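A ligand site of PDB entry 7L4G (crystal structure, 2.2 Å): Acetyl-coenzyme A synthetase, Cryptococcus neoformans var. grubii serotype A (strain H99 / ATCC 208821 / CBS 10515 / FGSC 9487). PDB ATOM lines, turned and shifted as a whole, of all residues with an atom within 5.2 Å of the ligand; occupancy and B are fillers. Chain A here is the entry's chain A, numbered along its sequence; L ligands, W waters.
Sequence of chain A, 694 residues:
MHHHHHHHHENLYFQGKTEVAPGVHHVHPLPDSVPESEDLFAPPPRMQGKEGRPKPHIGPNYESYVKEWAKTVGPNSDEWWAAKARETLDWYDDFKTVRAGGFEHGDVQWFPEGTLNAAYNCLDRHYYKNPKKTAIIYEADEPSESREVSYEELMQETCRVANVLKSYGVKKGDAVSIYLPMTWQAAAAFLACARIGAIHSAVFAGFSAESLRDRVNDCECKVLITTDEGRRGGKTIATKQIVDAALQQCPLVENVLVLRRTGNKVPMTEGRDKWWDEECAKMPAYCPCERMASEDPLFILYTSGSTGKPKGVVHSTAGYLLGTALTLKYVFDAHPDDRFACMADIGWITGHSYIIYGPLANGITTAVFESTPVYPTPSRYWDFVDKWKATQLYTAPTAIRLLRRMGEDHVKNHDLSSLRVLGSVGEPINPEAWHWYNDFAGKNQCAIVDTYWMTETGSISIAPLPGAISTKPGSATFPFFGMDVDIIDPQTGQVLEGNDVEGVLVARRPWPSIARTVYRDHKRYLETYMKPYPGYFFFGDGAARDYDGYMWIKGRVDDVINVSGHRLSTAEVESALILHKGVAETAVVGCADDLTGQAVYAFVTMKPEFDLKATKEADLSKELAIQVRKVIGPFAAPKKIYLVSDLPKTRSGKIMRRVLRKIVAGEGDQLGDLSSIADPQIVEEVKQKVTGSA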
ATOM      1  N   THR A 303     -27.071  25.207   6.728  1.00  0.00           N
ATOM      2  CA  THR A 303     -25.615  25.236   6.771  1.00  0.00           C
ATOM      3  C   THR A 303     -25.081  25.781   5.456  1.00  0.00           C
ATOM      4  O   THR A 303     -25.731  25.706   4.416  1.00  0.00           O
ATOM      5  CB  THR A 303     -25.053  23.850   7.030  1.00  0.00           C
ATOM      6  OG1 THR A 303     -25.472  22.978   5.974  1.00  0.00           O
ATOM      7  CG2 THR A 303     -25.566  23.316   8.342  1.00  0.00           C
ATOM      8  N   TRP A 348     -25.259  31.471  13.033  1.00  0.00           N
ATOM      9  CA  TRP A 348     -24.552  30.223  13.247  1.00  0.00           C
ATOM     10  C   TRP A 348     -25.255  29.432  14.344  1.00  0.00           C
ATOM     11  O   TRP A 348     -25.842  30.018  15.255  1.00  0.00           O
ATOM     12  CB  TRP A 348     -23.110  30.531  13.648  1.00  0.00           C
ATOM     13  CG  TRP A 348     -22.105  29.443  13.658  1.00  0.00           C
ATOM     14  CD1 TRP A 348     -22.179  28.211  13.045  1.00  0.00           C
ATOM     15  CD2 TRP A 348     -20.832  29.483  14.314  1.00  0.00           C
ATOM     16  NE1 TRP A 348     -21.030  27.489  13.277  1.00  0.00           N
ATOM     17  CE2 TRP A 348     -20.181  28.245  14.051  1.00  0.00           C
ATOM     18  CE3 TRP A 348     -20.167  30.449  15.079  1.00  0.00           C
ATOM     19  CZ2 TRP A 348     -18.899  27.954  14.541  1.00  0.00           C
ATOM     20  CZ3 TRP A 348     -18.885  30.158  15.569  1.00  0.00           C
ATOM     21  CH2 TRP A 348     -18.269  28.920  15.298  1.00  0.00           C
ATOM     22  N   ILE A 349     -25.174  28.097  14.277  1.00  0.00           N
ATOM     23  CA  ILE A 349     -25.741  27.283  15.366  1.00  0.00           C
ATOM     24  C   ILE A 349     -25.184  27.727  16.716  1.00  0.00           C
ATOM     25  O   ILE A 349     -25.916  27.701  17.727  1.00  0.00           O
ATOM     26  CB  ILE A 349     -25.485  25.781  15.114  1.00  0.00           C
ATOM     27  CG1 ILE A 349     -26.233  24.921  16.145  1.00  0.00           C
ATOM     28  CG2 ILE A 349     -23.995  25.451  15.115  1.00  0.00           C
ATOM     29  CD1 ILE A 349     -27.810  24.888  15.910  1.00  0.00           C
ATOM     30  N   THR A 350     -23.918  28.170  16.751  1.00  0.00           N
ATOM     31  CA  THR A 350     -23.315  28.617  18.001  1.00  0.00           C
ATOM     32  C   THR A 350     -24.110  29.770  18.626  1.00  0.00           C
ATOM     33  O   THR A 350     -24.306  29.802  19.845  1.00  0.00           O
ATOM     34  CB  THR A 350     -21.863  29.047  17.756  1.00  0.00           C
ATOM     35  OG1 THR A 350     -21.143  27.938  17.197  1.00  0.00           O
ATOM     36  CG2 THR A 350     -21.198  29.476  19.054  1.00  0.00           C
ATOM     37  N   SER A 424     -13.639  27.770  23.040  1.00  0.00           N
ATOM     38  CA  SER A 424     -13.293  27.877  21.631  1.00  0.00           C
ATOM     39  C   SER A 424     -14.155  26.882  20.869  1.00  0.00           C
ATOM     40  O   SER A 424     -14.265  25.724  21.271  1.00  0.00           O
ATOM     41  CB  SER A 424     -11.804  27.581  21.430  1.00  0.00           C
ATOM     42  OG  SER A 424     -11.488  27.482  20.069  1.00  0.00           O
ATOM     43  N   VAL A 425     -14.772  27.335  19.766  1.00  0.00           N
ATOM     44  CA  VAL A 425     -15.659  26.496  18.943  1.00  0.00           C
ATOM     45  C   VAL A 425     -15.423  26.798  17.466  1.00  0.00           C
ATOM     46  O   VAL A 425     -15.222  27.954  17.088  1.00  0.00           O
ATOM     47  CB  VAL A 425     -17.151  26.738  19.292  1.00  0.00           C
ATOM     48  CG1 VAL A 425     -17.493  28.215  19.174  1.00  0.00           C
ATOM     49  CG2 VAL A 425     -18.057  25.944  18.356  1.00  0.00           C
ATOM     50  N   GLY A 426     -15.503  25.759  16.627  1.00  0.00           N
ATOM     51  CA  GLY A 426     -15.640  25.964  15.198  1.00  0.00           C
ATOM     52  C   GLY A 426     -14.639  25.220  14.336  1.00  0.00           C
ATOM     53  O   GLY A 426     -14.903  24.923  13.163  1.00  0.00           O
ATOM     54  N   GLU A 427     -13.480  24.927  14.901  1.00  0.00           N
ATOM     55  CA  GLU A 427     -12.361  24.304  14.213  1.00  0.00           C
ATOM     56  C   GLU A 427     -11.375  23.833  15.278  1.00  0.00           C
ATOM     57  O   GLU A 427     -11.455  24.287  16.419  1.00  0.00           O
ATOM     58  CB  GLU A 427     -11.675  25.273  13.234  1.00  0.00           C
ATOM     59  CG  GLU A 427     -12.227  25.162  11.812  1.00  0.00           C
ATOM     60  CD  GLU A 427     -11.274  25.673  10.732  1.00  0.00           C
ATOM     61  OE1 GLU A 427     -10.223  26.283  11.088  1.00  0.00           O
ATOM     62  OE2 GLU A 427     -11.568  25.462   9.534  1.00  0.00           O
ATOM     63  N   PRO A 428     -10.470  22.932  14.929  1.00  0.00           N
ATOM     64  CA  PRO A 428      -9.371  22.619  15.858  1.00  0.00           C
ATOM     65  C   PRO A 428      -8.618  23.896  16.201  1.00  0.00           C
ATOM     66  O   PRO A 428      -8.348  24.732  15.335  1.00  0.00           O
ATOM     67  CB  PRO A 428      -8.499  21.640  15.064  1.00  0.00           C
ATOM     68  CG  PRO A 428      -9.472  21.041  14.017  1.00  0.00           C
ATOM     69  CD  PRO A 428     -10.389  22.155  13.674  1.00  0.00           C
ATOM     70  N   ASP A 450     -12.391  23.656  24.977  1.00  0.00           N
ATOM     71  CA  ASP A 450     -12.408  23.438  23.538  1.00  0.00           C
ATOM     72  C   ASP A 450     -13.651  22.596  23.227  1.00  0.00           C
ATOM     73  O   ASP A 450     -13.679  21.405  23.558  1.00  0.00           O
ATOM     74  CB  ASP A 450     -11.098  22.735  23.155  1.00  0.00           C
ATOM     75  CG  ASP A 450     -11.023  22.331  21.692  1.00  0.00           C
ATOM     76  OD1 ASP A 450     -11.907  22.674  20.898  1.00  0.00           O
ATOM     77  OD2 ASP A 450     -10.034  21.645  21.356  1.00  0.00           O
ATOM     78  N   THR A 451     -14.671  23.199  22.624  1.00  0.00           N
ATOM     79  CA  THR A 451     -15.998  22.577  22.505  1.00  0.00           C
ATOM     80  C   THR A 451     -16.212  22.094  21.068  1.00  0.00           C
ATOM     81  O   THR A 451     -16.386  22.904  20.148  1.00  0.00           O
ATOM     82  CB  THR A 451     -17.126  23.545  22.885  1.00  0.00           C
ATOM     83  OG1 THR A 451     -17.200  24.595  21.912  1.00  0.00           O
ATOM     84  CG2 THR A 451     -16.935  24.126  24.292  1.00  0.00           C
ATOM     85  N   TYR A 452     -16.233  20.770  20.892  1.00  0.00           N
ATOM     86  CA  TYR A 452     -16.475  20.174  19.589  1.00  0.00           C
ATOM     87  C   TYR A 452     -17.960  19.812  19.472  1.00  0.00           C
ATOM     88  O   TYR A 452     -18.519  19.156  20.357  1.00  0.00           O
ATOM     89  CB  TYR A 452     -15.600  18.942  19.391  1.00  0.00           C
ATOM     90  CG  TYR A 452     -16.044  18.119  18.199  1.00  0.00           C
ATOM     91  CD1 TYR A 452     -15.681  18.489  16.906  1.00  0.00           C
ATOM     92  CD2 TYR A 452     -16.869  17.016  18.363  1.00  0.00           C
ATOM     93  CE1 TYR A 452     -16.103  17.756  15.822  1.00  0.00           C
ATOM     94  CE2 TYR A 452     -17.291  16.273  17.277  1.00  0.00           C
ATOM     95  CZ  TYR A 452     -16.909  16.655  16.023  1.00  0.00           C
ATOM     96  OH  TYR A 452     -17.330  15.901  14.948  1.00  0.00           O
ATOM     97  N   TRP A 453     -18.591  20.252  18.380  1.00  0.00           N
ATOM     98  CA  TRP A 453     -19.962  19.882  18.040  1.00  0.00           C
ATOM     99  C   TRP A 453     -20.252  20.384  16.629  1.00  0.00           C
ATOM    100  O   TRP A 453     -19.346  20.871  15.926  1.00  0.00           O
ATOM    101  CB  TRP A 453     -20.990  20.429  19.047  1.00  0.00           C
ATOM    102  CG  TRP A 453     -20.968  21.909  19.264  1.00  0.00           C
ATOM    103  CD1 TRP A 453     -19.917  22.661  19.717  1.00  0.00           C
ATOM    104  CD2 TRP A 453     -22.054  22.828  19.077  1.00  0.00           C
ATOM    105  NE1 TRP A 453     -20.283  23.987  19.818  1.00  0.00           N
ATOM    106  CE2 TRP A 453     -21.591  24.113  19.422  1.00  0.00           C
ATOM    107  CE3 TRP A 453     -23.388  22.682  18.657  1.00  0.00           C
ATOM    108  CZ2 TRP A 453     -22.405  25.254  19.348  1.00  0.00           C
ATOM    109  CZ3 TRP A 453     -24.187  23.804  18.579  1.00  0.00           C
ATOM    110  CH2 TRP A 453     -23.694  25.074  18.907  1.00  0.00           C
ATOM    111  N   MET A 454     -21.513  20.214  16.191  1.00  0.00           N
ATOM    112  CA  MET A 454     -21.949  20.581  14.856  1.00  0.00           C
ATOM    113  C   MET A 454     -23.370  21.104  14.920  1.00  0.00           C
ATOM    114  O   MET A 454     -24.113  20.815  15.867  1.00  0.00           O
ATOM    115  CB  MET A 454     -21.928  19.418  13.854  1.00  0.00           C
ATOM    116  CG  MET A 454     -20.881  18.362  14.097  1.00  0.00           C
ATOM    117  SD  MET A 454     -20.750  17.274  12.681  1.00  0.00           S
ATOM    118  CE  MET A 454     -22.240  16.367  12.850  1.00  0.00           C
ATOM    119  N   THR A 455     -23.744  21.857  13.889  1.00  0.00           N
ATOM    120  CA  THR A 455     -25.124  22.267  13.684  1.00  0.00           C
ATOM    121  C   THR A 455     -26.040  21.068  13.890  1.00  0.00           C
ATOM    122  O   THR A 455     -27.063  21.174  14.575  1.00  0.00           O
ATOM    123  CB  THR A 455     -25.330  22.814  12.271  1.00  0.00           C
ATOM    124  OG1 THR A 455     -24.454  23.933  12.047  1.00  0.00           O
ATOM    125  CG2 THR A 455     -26.769  23.267  12.088  1.00  0.00           C
ATOM    126  N   GLU A 456     -25.651  19.921  13.350  1.00  0.00           N
ATOM    127  CA  GLU A 456     -26.492  18.733  13.430  1.00  0.00           C
ATOM    128  C   GLU A 456     -26.502  18.080  14.821  1.00  0.00           C
ATOM    129  O   GLU A 456     -27.382  17.248  15.087  1.00  0.00           O
ATOM    130  CB  GLU A 456     -26.049  17.697  12.395  1.00  0.00           C
ATOM    131  CG  GLU A 456     -26.167  18.175  10.940  1.00  0.00           C
ATOM    132  CD  GLU A 456     -24.885  18.861  10.428  1.00  0.00           C
ATOM    133  OE1 GLU A 456     -24.159  19.474  11.225  1.00  0.00           O
ATOM    134  OE2 GLU A 456     -24.587  18.760   9.211  1.00  0.00           O
ATOM    135  N   PHE A 539     -20.058  11.943  12.076  1.00  0.00           N
ATOM    136  CA  PHE A 539     -19.839  13.389  12.153  1.00  0.00           C
ATOM    137  C   PHE A 539     -19.173  13.948  10.895  1.00  0.00           C
ATOM    138  O   PHE A 539     -19.344  15.132  10.601  1.00  0.00           O
ATOM    139  CB  PHE A 539     -18.949  13.757  13.350  1.00  0.00           C
ATOM    140  CG  PHE A 539     -19.573  13.530  14.697  1.00  0.00           C
ATOM    141  CD1 PHE A 539     -19.508  12.285  15.294  1.00  0.00           C
ATOM    142  CD2 PHE A 539     -20.174  14.574  15.382  1.00  0.00           C
ATOM    143  CE1 PHE A 539     -20.059  12.081  16.546  1.00  0.00           C
ATOM    144  CE2 PHE A 539     -20.732  14.381  16.629  1.00  0.00           C
ATOM    145  CZ  PHE A 539     -20.689  13.137  17.219  1.00  0.00           C
ATOM    146  N   ASP A 541     -15.780  14.003  10.753  1.00  0.00           N
ATOM    147  CA  ASP A 541     -14.480  14.484  11.225  1.00  0.00           C
ATOM    148  C   ASP A 541     -13.538  13.320  11.521  1.00  0.00           C
ATOM    149  O   ASP A 541     -13.967  12.287  12.044  1.00  0.00           O
ATOM    150  CB  ASP A 541     -14.641  15.329  12.486  1.00  0.00           C
ATOM    151  CG  ASP A 541     -15.377  16.637  12.226  1.00  0.00           C
ATOM    152  OD1 ASP A 541     -14.788  17.489  11.530  1.00  0.00           O
ATOM    153  OD2 ASP A 541     -16.550  16.786  12.686  1.00  0.00           O
ATOM    154  N   ILE A 553      -9.952  15.929  17.906  1.00  0.00           N
ATOM    155  CA  ILE A 553     -10.632  16.121  16.621  1.00  0.00           C
ATOM    156  C   ILE A 553      -9.638  16.750  15.661  1.00  0.00           C
ATOM    157  O   ILE A 553      -9.236  17.892  15.857  1.00  0.00           O
ATOM    158  CB  ILE A 553     -11.869  17.005  16.755  1.00  0.00           C
ATOM    159  CG1 ILE A 553     -12.734  16.549  17.930  1.00  0.00           C
ATOM    160  CG2 ILE A 553     -12.631  16.969  15.424  1.00  0.00           C
ATOM    161  CD1 ILE A 553     -13.192  15.126  17.793  1.00  0.00           C
ATOM    162  N   GLY A 555      -9.748  17.278  12.204  1.00  0.00           N
ATOM    163  CA  GLY A 555     -10.171  17.956  10.996  1.00  0.00           C
ATOM    164  C   GLY A 555     -11.195  17.150  10.228  1.00  0.00           C
ATOM    165  O   GLY A 555     -11.545  16.030  10.603  1.00  0.00           O
ATOM    166  N   ARG A 556     -11.675  17.737   9.143  1.00  0.00           N
ATOM    167  CA  ARG A 556     -12.696  17.108   8.320  1.00  0.00           C
ATOM    168  C   ARG A 556     -12.116  15.896   7.597  1.00  0.00           C
ATOM    169  O   ARG A 556     -10.976  15.911   7.129  1.00  0.00           O
ATOM    170  CB  ARG A 556     -13.261  18.092   7.276  1.00  0.00           C
ATOM    171  CG  ARG A 556     -14.221  19.177   7.810  1.00  0.00           C
ATOM    172  CD  ARG A 556     -15.462  18.590   8.482  1.00  0.00           C
ATOM    173  NE  ARG A 556     -16.500  18.137   7.553  1.00  0.00           N
ATOM    174  CZ  ARG A 556     -17.610  17.516   7.939  1.00  0.00           C
ATOM    175  NH1 ARG A 556     -17.855  17.269   9.211  1.00  0.00           N
ATOM    176  NH2 ARG A 556     -18.503  17.161   7.013  1.00  0.00           N
ATOM    177  N   SER A 652     -18.888  32.041   9.588  1.00  0.00           N
ATOM    178  CA  SER A 652     -18.640  31.410  10.875  1.00  0.00           C
ATOM    179  C   SER A 652     -17.153  31.145  11.144  1.00  0.00           C
ATOM    180  O   SER A 652     -16.821  30.573  12.178  1.00  0.00           O
ATOM    181  CB  SER A 652     -19.442  30.092  10.992  1.00  0.00           C
ATOM    182  OG  SER A 652     -18.873  29.031  10.237  1.00  0.00           O
HETATM  183  C1  LIG L   1     -20.513  24.369  16.253  1.00  0.00           C
HETATM  184  C2  LIG L   1     -20.061  24.317  14.798  1.00  0.00           C
HETATM  185  C3  LIG L   1     -19.205  21.707  12.463  1.00  0.00           C
HETATM  186  C4  LIG L   1     -17.760  21.396  12.091  1.00  0.00           C
HETATM  187  C5  LIG L   1     -17.362  20.045  12.767  1.00  0.00           C
HETATM  188  C6  LIG L   1     -15.838  20.167  12.817  1.00  0.00           C
HETATM  189  C7  LIG L   1     -15.657  21.467  13.086  1.00  0.00           C
HETATM  190  C8  LIG L   1     -16.386  22.649  15.182  1.00  0.00           C
HETATM  191  C9  LIG L   1     -14.734  22.134  16.479  1.00  0.00           C
HETATM  192  C10 LIG L   1     -14.526  21.564  15.236  1.00  0.00           C
HETATM  193  C11 LIG L   1     -12.543  20.619  15.940  1.00  0.00           C
HETATM  194  C12 LIG L   1     -13.738  21.890  17.450  1.00  0.00           C
HETATM  195  N1  LIG L   1     -15.553  21.916  14.470  1.00  0.00           N
HETATM  196  N2  LIG L   1     -15.894  22.808  16.417  1.00  0.00           N
HETATM  197  N3  LIG L   1     -13.432  20.823  14.985  1.00  0.00           N
HETATM  198  N4  LIG L   1     -12.698  21.150  17.139  1.00  0.00           N
HETATM  199  N5  LIG L   1     -13.849  22.445  18.778  1.00  0.00           N
HETATM  200  O1  LIG L   1     -18.936  24.581  14.544  1.00  0.00           O
HETATM  201  O2  LIG L   1     -21.029  23.959  13.818  1.00  0.00           O
HETATM  202  O3  LIG L   1     -20.725  25.140  11.522  1.00  0.00           O
HETATM  203  O4  LIG L   1     -21.889  22.927  11.687  1.00  0.00           O
HETATM  204  O5  LIG L   1     -19.339  23.005  11.985  1.00  0.00           O
HETATM  205  O6  LIG L   1     -16.957  22.294  12.627  1.00  0.00           O
HETATM  206  O7  LIG L   1     -15.250  19.857  11.576  1.00  0.00           O
HETATM  207  O8  LIG L   1     -17.768  18.983  11.973  1.00  0.00           O
HETATM  208  P1  LIG L   1     -20.751  23.798  12.175  1.00  0.00           P
HETATM  209  O   HOH W   1     -11.593  24.930  19.164  1.00  0.00           O
HETATM  210  O   HOH W   2     -11.409  20.023  19.574  1.00  0.00           O
HETATM  211  O   HOH W   3     -22.204  20.857   9.992  1.00  0.00           O
HETATM  212  O   HOH W   4     -17.362  25.191  11.675  1.00  0.00           O
HETATM  213  O   HOH W   5     -12.638  19.178  12.492  1.00  0.00           O
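OD1 of Asp 541 sits at hydrogen-bond distance from O7 of the ligand (2.4 Å).
O4 of the ligand lies within hydrogen-bond range of N of Thr 455.
An oxygen (O4) of the ligand lies within hydrogen-bond range of the side-chain hydroxyl (OG1) of Thr 455 (2.8 Å).
N5 of the ligand lies within hydrogen-bond range of OD1 of Asp 450, at 2.9 Å.
The backbone carbonyl oxygen (O) of Thr 451 lies within hydrogen-bond range of a nitrogen (N5) of the ligand.
NE1 of Trp 348 lies within hydrogen-bond range of O3 of the ligand (2.9 Å).
N of Gly 426 is in hydrogen-bond range of N2 of the ligand (3.0 Å).
NH1 of Arg 556 sits at hydrogen-bond distance from O8 of the ligand.
SD of Met 454 sits at hydrogen-bond distance from O8 of the ligand (3.5 Å).
The side-chain carboxylate (OD2) of Asp 541 lies within salt-bridge range of the guanidinium group (NH1) of Arg 556 (3.7 Å).
OD2 of Asp 541 sits at hydrogen-bond distance from OH of Tyr 452, 2.6 Å away.
N of Thr 451 is in hydrogen-bond range of O of Ser 424 (2.9 Å).
The guanidinium group of Arg 556 lies within hydrogen-bond range of the backbone carbonyl oxygen of Phe 539, at 3.0 Å.
The backbone carbonyl oxygen (O) of Glu 427 lies close to a nitrogen (N4) of the ligand (3.5 Å).
Ile 349 touches the ligand (CG2 to O2, 3.6 Å).
Thr 350 touches the ligand.
Val 425 touches the ligand.
Pro 428 touches the ligand.
Tyr 452 touches the ligand (CA to N5, 3.6 Å).
CE2 of Trp 453 touches C1 of the ligand, at 3.4 Å.
Ile 553 touches the ligand.
Hydrophobic or aromatic side chains that line the ligand: Trp 348, Ile 349, Val 425, Pro 428, Tyr 452, Trp 453, Met 454 and Ile 553.
Of the 22 residues printed, 16 come within 4 Å of the ligand.
Along chain A the residues within 4 Å of the ligand span positions 348 to 556.
Water W3 lies within hydrogen-bond range of an oxygen (O4) of the ligand and the side-chain carboxylate of Glu 456.
Water W5 lies within hydrogen-bond range of O7 of the ligand (2.9 Å), OD1 of Asp 541 (2.9 Å) and N of Gly 555 (3.5 Å).
Water W4 bridges O of Gly 426 and O5 of the ligand.
Water W2 lies within hydrogen-bond range of the side-chain carboxylate of Asp 450 (2.8 Å) and a nitrogen (N4) of the ligand (3.0 Å).
Water W1 lies within hydrogen-bond range of the side-chain hydroxyl of Ser 424 (2.7 Å), the backbone carbonyl oxygen of Glu 427 (2.8 Å), the side-chain carboxylate of Asp 450 (2.9 Å) and a nitrogen (N5) of the ligand (3.4 Å).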
